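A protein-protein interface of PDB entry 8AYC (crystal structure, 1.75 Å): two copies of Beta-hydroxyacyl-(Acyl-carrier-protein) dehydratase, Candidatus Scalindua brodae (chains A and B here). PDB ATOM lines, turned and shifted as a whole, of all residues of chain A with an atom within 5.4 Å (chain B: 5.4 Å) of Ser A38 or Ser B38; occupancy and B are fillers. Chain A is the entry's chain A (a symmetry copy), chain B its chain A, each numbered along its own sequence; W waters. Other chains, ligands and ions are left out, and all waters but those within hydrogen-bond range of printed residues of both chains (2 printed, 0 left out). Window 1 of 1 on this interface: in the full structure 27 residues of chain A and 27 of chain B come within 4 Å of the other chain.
Printed residues of chain B within 4 Å of Ile A37: Asn B36 (2.9 Å). Ser A38 touches five residues of chain B. Printed residues of chain B within 4 Å of Gly A101: Asp B20 (3.7 Å) and Asn B36 (3.1 Å). Of the printed residues of chain A, Lys B35 touches Ser A38 (3.7 Å). Of chain A, only Asp A20 (3.7 Å), Lys A35 (3.7 Å), Asn A36 (3.7 Å), Ser A38 (3.8 Å) and Glu A41 (3.6 Å) come within 4 Å of Ser B38. The nearest residue of chain A that does not touch Ser B38 is Ile A37 (5.3 Å).
Of the 11 printed residues of chain A, 10 touch a printed residue of chain B. Printed residues of chain A that touch a printed residue of chain B: Asp A20, Lys A35, Asn A36, Ile A37, Ser A38, Gly A39, Asn A40, Glu A41, Pro A100 and Gly A101. Hydrophobic or aromatic side chains of chain A within 4 Å of the printed part of chain B: Pro A100. Along chain A the printed residues that touch a printed residue of chain B span positions 20 to 101. Hydrophobic or aromatic side chains of chain B that line the printed part of chain A: Pro B100. Among the printed residues, no Asp or Glu carboxylate lies within 4 Å of a Lys or Arg side-chain nitrogen of the other chain.
The side-chain amide nitrogen of Asn B36 is in hydrogen-bond range of the backbone carbonyl oxygen of Ile A37 (2.9 Å). ND2 of Asn A36 lies within hydrogen-bond range of O of Ile B37 (2.9 Å). The backbone NH (N) of Gly B39 is in hydrogen-bond range of the side-chain carboxylate (OD1) of Asp A20 (2.7 Å). The side-chain amide nitrogen (ND2) of Asn B40 sits at hydrogen-bond distance from the side-chain carboxylate (OE1) of Glu A41 (3.0 Å). The side-chain carboxylate (OE1) of Glu B41 lies within hydrogen-bond range of the side-chain amide nitrogen (ND2) of Asn A40, 3.0 Å away. The side-chain amide nitrogen (ND2) of Asn B36 lies close to the backbone carbonyl oxygen (O) of Gly A101. O of Gly B101 lies close to ND2 of Asn A36, at 3.2 Å. OD1 of Asp B20 lies within hydrogen-bond range of N of Gly A39 (2.7 Å).
Water W1 lies within hydrogen-bond range of OG of Ser A38, OD2 of Asp B20, NZ of Lys B35 and O of Asn B36. Water W2 lies within hydrogen-bond range of OG of Ser B38 (2.6 Å), OD2 of Asp A20 (2.6 Å), NZ of Lys A35 (2.8 Å) and O of Asn A36 (3.4 Å).
Asp A20 touches Gly B39, and with the chains exchanged Gly A39 touches Asp B20. Asp A20 touches Pro B100, and with the chains exchanged Pro A100 touches Asp B20. Lys A35 touches Ser B38, and with the chains exchanged Ser A38 touches Lys B35. Asn A40 touches Glu B41, and with the chains exchanged Glu A41 touches Asn B40. Of the 22 pairs that touch across the chains among the printed residues, 22 have their exchanged pair printed and touching as well.
The backbone carbonyl oxygen of Ile B37 lies within hydrogen-bond range of the backbone NH of Gly B101 (2.9 Å). OD2 of Asp A20 is in hydrogen-bond range of N of Asn A36, 2.8 Å away. OG of Ser B38 lies within hydrogen-bond range of N of Asn B40. The side-chain carboxylate (OE1) of Glu A41 lies within salt-bridge range of the side-chain amino group (NZ) of Lys A35 (2.8 Å). The side-chain carboxylate (OE2) of Glu B41 is in hydrogen-bond range of the backbone NH (N) of Ser B38 (2.8 Å). OG of Ser A38 sits at hydrogen-bond distance from N of Asn A40, at 3.0 Å.
Among the printed residues, merely in contact across the chains: Glu A41 with Ser B38 (3.6 Å), Ser A38 with Glu B41 (3.6 Å), Pro A100 with Asp B20 (3.7 Å), Asp A20 with Pro B100 (3.7 Å), Ser A38 with Lys B35 (3.7 Å), Lys A35 with Ser B38 (3.7 Å), Asn A36 with Ser B38 (3.7 Å), Ser A38 with Asn B36 (3.7 Å), Asp A20 with Ser B38 (3.7 Å), Ser A38 with Asp B20 (3.7 Å), Gly A101 with Asp B20 (3.7 Å), Asp A20 with Gly B101 (3.7 Å), Ser A38 with Ser B38 (3.8 Å) and Asn A36 with Asn B36 (3.9 Å).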
ATOM      1  N   ASP A  20      -3.028  -0.582   8.252  1.00  0.00           N
ATOM      2  CA  ASP A  20      -3.381  -1.550   7.219  1.00  0.00           C
ATOM      3  C   ASP A  20      -2.943  -1.103   5.826  1.00  0.00           C
ATOM      4  O   ASP A  20      -2.385  -1.902   5.076  1.00  0.00           O
ATOM      5  CB  ASP A  20      -4.890  -1.833   7.231  1.00  0.00           C
ATOM      6  CG  ASP A  20      -5.292  -2.678   8.405  1.00  0.00           C
ATOM      7  OD1 ASP A  20      -4.658  -3.741   8.611  1.00  0.00           O
ATOM      8  OD2 ASP A  20      -6.198  -2.268   9.150  1.00  0.00           O
ATOM      9  N   LYS A  35      -6.436   2.401   9.158  1.00  0.00           N
ATOM     10  CA  LYS A  35      -6.445   1.228  10.026  1.00  0.00           C
ATOM     11  C   LYS A  35      -7.886   0.773  10.226  1.00  0.00           C
ATOM     12  O   LYS A  35      -8.695   1.504  10.809  1.00  0.00           O
ATOM     13  CB  LYS A  35      -5.789   1.505  11.381  1.00  0.00           C
ATOM     14  CG  LYS A  35      -5.762   0.219  12.229  1.00  0.00           C
ATOM     15  CD  LYS A  35      -5.830   0.483  13.711  1.00  0.00           C
ATOM     16  CE  LYS A  35      -5.680  -0.825  14.496  1.00  0.00           C
ATOM     17  NZ  LYS A  35      -6.451  -1.926  13.903  1.00  0.00           N
ATOM     18  N   ASN A  36      -8.208  -0.428   9.740  1.00  0.00           N
ATOM     19  CA  ASN A  36      -9.501  -1.027  10.053  1.00  0.00           C
ATOM     20  C   ASN A  36      -9.551  -1.420  11.526  1.00  0.00           C
ATOM     21  O   ASN A  36      -8.602  -2.013  12.063  1.00  0.00           O
ATOM     22  CB  ASN A  36      -9.761  -2.264   9.190  1.00  0.00           C
ATOM     23  CG  ASN A  36     -10.293  -1.932   7.811  1.00  0.00           C
ATOM     24  OD1 ASN A  36     -10.741  -0.816   7.546  1.00  0.00           O
ATOM     25  ND2 ASN A  36     -10.265  -2.914   6.923  1.00  0.00           N
ATOM     26  N   ILE A  37     -10.657  -1.088  12.191  1.00  0.00           N
ATOM     27  CA  ILE A  37     -10.885  -1.513  13.573  1.00  0.00           C
ATOM     28  C   ILE A  37     -11.769  -2.751  13.540  1.00  0.00           C
ATOM     29  O   ILE A  37     -12.913  -2.694  13.070  1.00  0.00           O
ATOM     30  CB  ILE A  37     -11.523  -0.401  14.422  1.00  0.00           C
ATOM     31  CG1 ILE A  37     -10.798   0.937  14.229  1.00  0.00           C
ATOM     32  CG2 ILE A  37     -11.554  -0.801  15.900  1.00  0.00           C
ATOM     33  CD1 ILE A  37      -9.287   0.892  14.467  1.00  0.00           C
ATOM     34  N   SER A  38     -11.250  -3.871  14.045  1.00  0.00           N
ATOM     35  CA  SER A  38     -11.943  -5.152  13.999  1.00  0.00           C
ATOM     36  C   SER A  38     -12.181  -5.683  15.405  1.00  0.00           C
ATOM     37  O   SER A  38     -11.276  -5.678  16.247  1.00  0.00           O
ATOM     38  CB  SER A  38     -11.128  -6.180  13.190  1.00  0.00           C
ATOM     39  OG  SER A  38     -11.600  -7.506  13.422  1.00  0.00           O
ATOM     40  N   GLY A  39     -13.391  -6.192  15.644  1.00  0.00           N
ATOM     41  CA  GLY A  39     -13.666  -6.856  16.909  1.00  0.00           C
ATOM     42  C   GLY A  39     -12.807  -8.081  17.172  1.00  0.00           C
ATOM     43  O   GLY A  39     -12.811  -8.587  18.298  1.00  0.00           O
ATOM     44  N   ASN A  40     -12.086  -8.573  16.164  1.00  0.00           N
ATOM     45  CA  ASN A  40     -11.242  -9.754  16.306  1.00  0.00           C
ATOM     46  C   ASN A  40      -9.781  -9.384  16.579  1.00  0.00           C
ATOM     47  O   ASN A  40      -8.891 -10.242  16.467  1.00  0.00           O
ATOM     48  CB  ASN A  40     -11.361 -10.624  15.046  1.00  0.00           C
ATOM     49  CG  ASN A  40     -10.756 -12.010  15.220  1.00  0.00           C
ATOM     50  OD1 ASN A  40     -10.952 -12.675  16.244  1.00  0.00           O
ATOM     51  ND2 ASN A  40     -10.005 -12.448  14.207  1.00  0.00           N
ATOM     52  N   GLU A  41      -9.515  -8.129  16.964  1.00  0.00           N
ATOM     53  CA  GLU A  41      -8.172  -7.732  17.407  1.00  0.00           C
ATOM     54  C   GLU A  41      -7.977  -8.063  18.886  1.00  0.00           C
ATOM     55  O   GLU A  41      -8.913  -7.916  19.683  1.00  0.00           O
ATOM     56  CB  GLU A  41      -7.958  -6.248  17.174  1.00  0.00           C
ATOM     57  CG  GLU A  41      -8.039  -5.867  15.699  1.00  0.00           C
ATOM     58  CD  GLU A  41      -7.724  -4.422  15.462  1.00  0.00           C
ATOM     59  OE1 GLU A  41      -6.568  -4.021  15.692  1.00  0.00           O
ATOM     60  OE2 GLU A  41      -8.627  -3.669  15.028  1.00  0.00           O
ATOM     61  N   PHE A  44      -9.110  -5.926  22.226  1.00  0.00           N
ATOM     62  CA  PHE A  44     -10.490  -5.635  22.616  1.00  0.00           C
ATOM     63  C   PHE A  44     -10.958  -6.501  23.776  1.00  0.00           C
ATOM     64  O   PHE A  44     -11.786  -6.052  24.583  1.00  0.00           O
ATOM     65  CB  PHE A  44     -11.420  -5.780  21.413  1.00  0.00           C
ATOM     66  CG  PHE A  44     -11.487  -4.533  20.567  1.00  0.00           C
ATOM     67  CD1 PHE A  44     -11.878  -3.319  21.135  1.00  0.00           C
ATOM     68  CD2 PHE A  44     -11.152  -4.566  19.217  1.00  0.00           C
ATOM     69  CE1 PHE A  44     -11.943  -2.156  20.365  1.00  0.00           C
ATOM     70  CE2 PHE A  44     -11.215  -3.409  18.436  1.00  0.00           C
ATOM     71  CZ  PHE A  44     -11.615  -2.199  19.020  1.00  0.00           C
ATOM     72  N   PRO A 100     -15.221  -1.342  17.084  1.00  0.00           N
ATOM     73  CA  PRO A 100     -15.205  -2.361  16.024  1.00  0.00           C
ATOM     74  C   PRO A 100     -16.167  -2.023  14.893  1.00  0.00           C
ATOM     75  O   PRO A 100     -17.334  -1.691  15.120  1.00  0.00           O
ATOM     76  CB  PRO A 100     -15.634  -3.631  16.767  1.00  0.00           C
ATOM     77  CG  PRO A 100     -15.125  -3.411  18.160  1.00  0.00           C
ATOM     78  CD  PRO A 100     -15.351  -1.945  18.422  1.00  0.00           C
ATOM     79  N   GLY A 101     -15.683  -2.138  13.659  1.00  0.00           N
ATOM     80  CA  GLY A 101     -16.452  -1.756  12.490  1.00  0.00           C
ATOM     81  C   GLY A 101     -16.110  -0.380  11.950  1.00  0.00           C
ATOM     82  O   GLY A 101     -16.428  -0.091  10.790  1.00  0.00           O
ATOM     83  N   ASP B  20     -18.549  -7.496  12.606  1.00  0.00           N
ATOM     84  CA  ASP B  20     -18.395  -6.257  13.361  1.00  0.00           C
ATOM     85  C   ASP B  20     -19.714  -5.505  13.522  1.00  0.00           C
ATOM     86  O   ASP B  20     -20.024  -5.043  14.620  1.00  0.00           O
ATOM     87  CB  ASP B  20     -17.345  -5.348  12.707  1.00  0.00           C
ATOM     88  CG  ASP B  20     -15.950  -5.858  12.924  1.00  0.00           C
ATOM     89  OD1 ASP B  20     -15.600  -6.137  14.096  1.00  0.00           O
ATOM     90  OD2 ASP B  20     -15.219  -6.029  11.933  1.00  0.00           O
ATOM     91  N   LYS B  35     -17.718  -6.967   8.096  1.00  0.00           N
ATOM     92  CA  LYS B  35     -16.544  -7.382   8.856  1.00  0.00           C
ATOM     93  C   LYS B  35     -15.327  -6.621   8.342  1.00  0.00           C
ATOM     94  O   LYS B  35     -14.930  -6.791   7.184  1.00  0.00           O
ATOM     95  CB  LYS B  35     -16.297  -8.890   8.766  1.00  0.00           C
ATOM     96  CG  LYS B  35     -15.092  -9.283   9.642  1.00  0.00           C
ATOM     97  CD  LYS B  35     -14.341 -10.478   9.116  1.00  0.00           C
ATOM     98  CE  LYS B  35     -13.232 -10.886  10.092  1.00  0.00           C
ATOM     99  NZ  LYS B  35     -12.503  -9.728  10.627  1.00  0.00           N
ATOM    100  N   ASN B  36     -14.743  -5.779   9.196  1.00  0.00           N
ATOM    101  CA  ASN B  36     -13.465  -5.158   8.862  1.00  0.00           C
ATOM    102  C   ASN B  36     -12.358  -6.207   8.870  1.00  0.00           C
ATOM    103  O   ASN B  36     -12.265  -7.033   9.789  1.00  0.00           O
ATOM    104  CB  ASN B  36     -13.114  -4.045   9.852  1.00  0.00           C
ATOM    105  CG  ASN B  36     -13.793  -2.727   9.537  1.00  0.00           C
ATOM    106  OD1 ASN B  36     -14.316  -2.518   8.443  1.00  0.00           O
ATOM    107  ND2 ASN B  36     -13.770  -1.815  10.497  1.00  0.00           N
ATOM    108  N   ILE B  37     -11.513  -6.183   7.839  1.00  0.00           N
ATOM    109  CA  ILE B  37     -10.336  -7.052   7.785  1.00  0.00           C
ATOM    110  C   ILE B  37      -9.137  -6.242   8.258  1.00  0.00           C
ATOM    111  O   ILE B  37      -8.773  -5.236   7.636  1.00  0.00           O
ATOM    112  CB  ILE B  37     -10.098  -7.617   6.376  1.00  0.00           C
ATOM    113  CG1 ILE B  37     -11.392  -8.180   5.773  1.00  0.00           C
ATOM    114  CG2 ILE B  37      -8.995  -8.680   6.397  1.00  0.00           C
ATOM    115  CD1 ILE B  37     -12.111  -9.214   6.642  1.00  0.00           C
ATOM    116  N   SER B  38      -8.513  -6.681   9.352  1.00  0.00           N
ATOM    117  CA  SER B  38      -7.410  -5.959   9.974  1.00  0.00           C
ATOM    118  C   SER B  38      -6.152  -6.817   9.993  1.00  0.00           C
ATOM    119  O   SER B  38      -6.196  -7.997  10.358  1.00  0.00           O
ATOM    120  CB  SER B  38      -7.775  -5.545  11.413  1.00  0.00           C
ATOM    121  OG  SER B  38      -6.613  -5.159  12.146  1.00  0.00           O
ATOM    122  N   GLY B  39      -5.018  -6.205   9.649  1.00  0.00           N
ATOM    123  CA  GLY B  39      -3.746  -6.900   9.779  1.00  0.00           C
ATOM    124  C   GLY B  39      -3.403  -7.314  11.199  1.00  0.00           C
ATOM    125  O   GLY B  39      -2.460  -8.089  11.387  1.00  0.00           O
ATOM    126  N   ASN B  40      -4.131  -6.812  12.195  1.00  0.00           N
ATOM    127  CA  ASN B  40      -3.873  -7.132  13.596  1.00  0.00           C
ATOM    128  C   ASN B  40      -4.780  -8.260  14.100  1.00  0.00           C
ATOM    129  O   ASN B  40      -4.879  -8.479  15.318  1.00  0.00           O
ATOM    130  CB  ASN B  40      -4.044  -5.867  14.451  1.00  0.00           C
ATOM    131  CG  ASN B  40      -3.513  -6.031  15.867  1.00  0.00           C
ATOM    132  OD1 ASN B  40      -2.427  -6.580  16.089  1.00  0.00           O
ATOM    133  ND2 ASN B  40      -4.292  -5.554  16.840  1.00  0.00           N
ATOM    134  N   GLU B  41      -5.421  -9.002  13.189  1.00  0.00           N
ATOM    135  CA  GLU B  41      -6.175 -10.205  13.572  1.00  0.00           C
ATOM    136  C   GLU B  41      -5.241 -11.410  13.672  1.00  0.00           C
ATOM    137  O   GLU B  41      -4.314 -11.546  12.862  1.00  0.00           O
ATOM    138  CB  GLU B  41      -7.275 -10.480  12.564  1.00  0.00           C
ATOM    139  CG  GLU B  41      -8.299  -9.352  12.491  1.00  0.00           C
ATOM    140  CD  GLU B  41      -9.440  -9.673  11.574  1.00  0.00           C
ATOM    141  OE1 GLU B  41     -10.209 -10.601  11.886  1.00  0.00           O
ATOM    142  OE2 GLU B  41      -9.590  -8.990  10.533  1.00  0.00           O
ATOM    143  N   PHE B  44      -3.848 -13.903  10.696  1.00  0.00           N
ATOM    144  CA  PHE B  44      -2.978 -13.497   9.592  1.00  0.00           C
ATOM    145  C   PHE B  44      -1.541 -13.953   9.788  1.00  0.00           C
ATOM    146  O   PHE B  44      -0.842 -14.227   8.801  1.00  0.00           O
ATOM    147  CB  PHE B  44      -3.052 -11.984   9.390  1.00  0.00           C
ATOM    148  CG  PHE B  44      -4.210 -11.561   8.521  1.00  0.00           C
ATOM    149  CD1 PHE B  44      -4.338 -12.068   7.226  1.00  0.00           C
ATOM    150  CD2 PHE B  44      -5.172 -10.675   8.995  1.00  0.00           C
ATOM    151  CE1 PHE B  44      -5.406 -11.686   6.411  1.00  0.00           C
ATOM    152  CE2 PHE B  44      -6.243 -10.284   8.187  1.00  0.00           C
ATOM    153  CZ  PHE B  44      -6.355 -10.796   6.888  1.00  0.00           C
ATOM    154  N   PRO B 100      -5.857  -7.418   4.475  1.00  0.00           N
ATOM    155  CA  PRO B 100      -5.905  -6.355   5.488  1.00  0.00           C
ATOM    156  C   PRO B 100      -6.191  -4.991   4.873  1.00  0.00           C
ATOM    157  O   PRO B 100      -5.564  -4.587   3.890  1.00  0.00           O
ATOM    158  CB  PRO B 100      -4.503  -6.410   6.107  1.00  0.00           C
ATOM    159  CG  PRO B 100      -4.116  -7.852   5.969  1.00  0.00           C
ATOM    160  CD  PRO B 100      -4.661  -8.267   4.627  1.00  0.00           C
ATOM    161  N   GLY B 101      -7.126  -4.262   5.476  1.00  0.00           N
ATOM    162  CA  GLY B 101      -7.572  -2.989   4.944  1.00  0.00           C
ATOM    163  C   GLY B 101      -8.864  -3.070   4.155  1.00  0.00           C
ATOM    164  O   GLY B 101      -9.516  -2.035   3.957  1.00  0.00           O
HETATM  165  O   HOH W   1     -13.919  -8.253  12.531  1.00  0.00           O
HETATM  166  O   HOH W   2      -5.352  -2.969  11.556  1.00  0.00           O
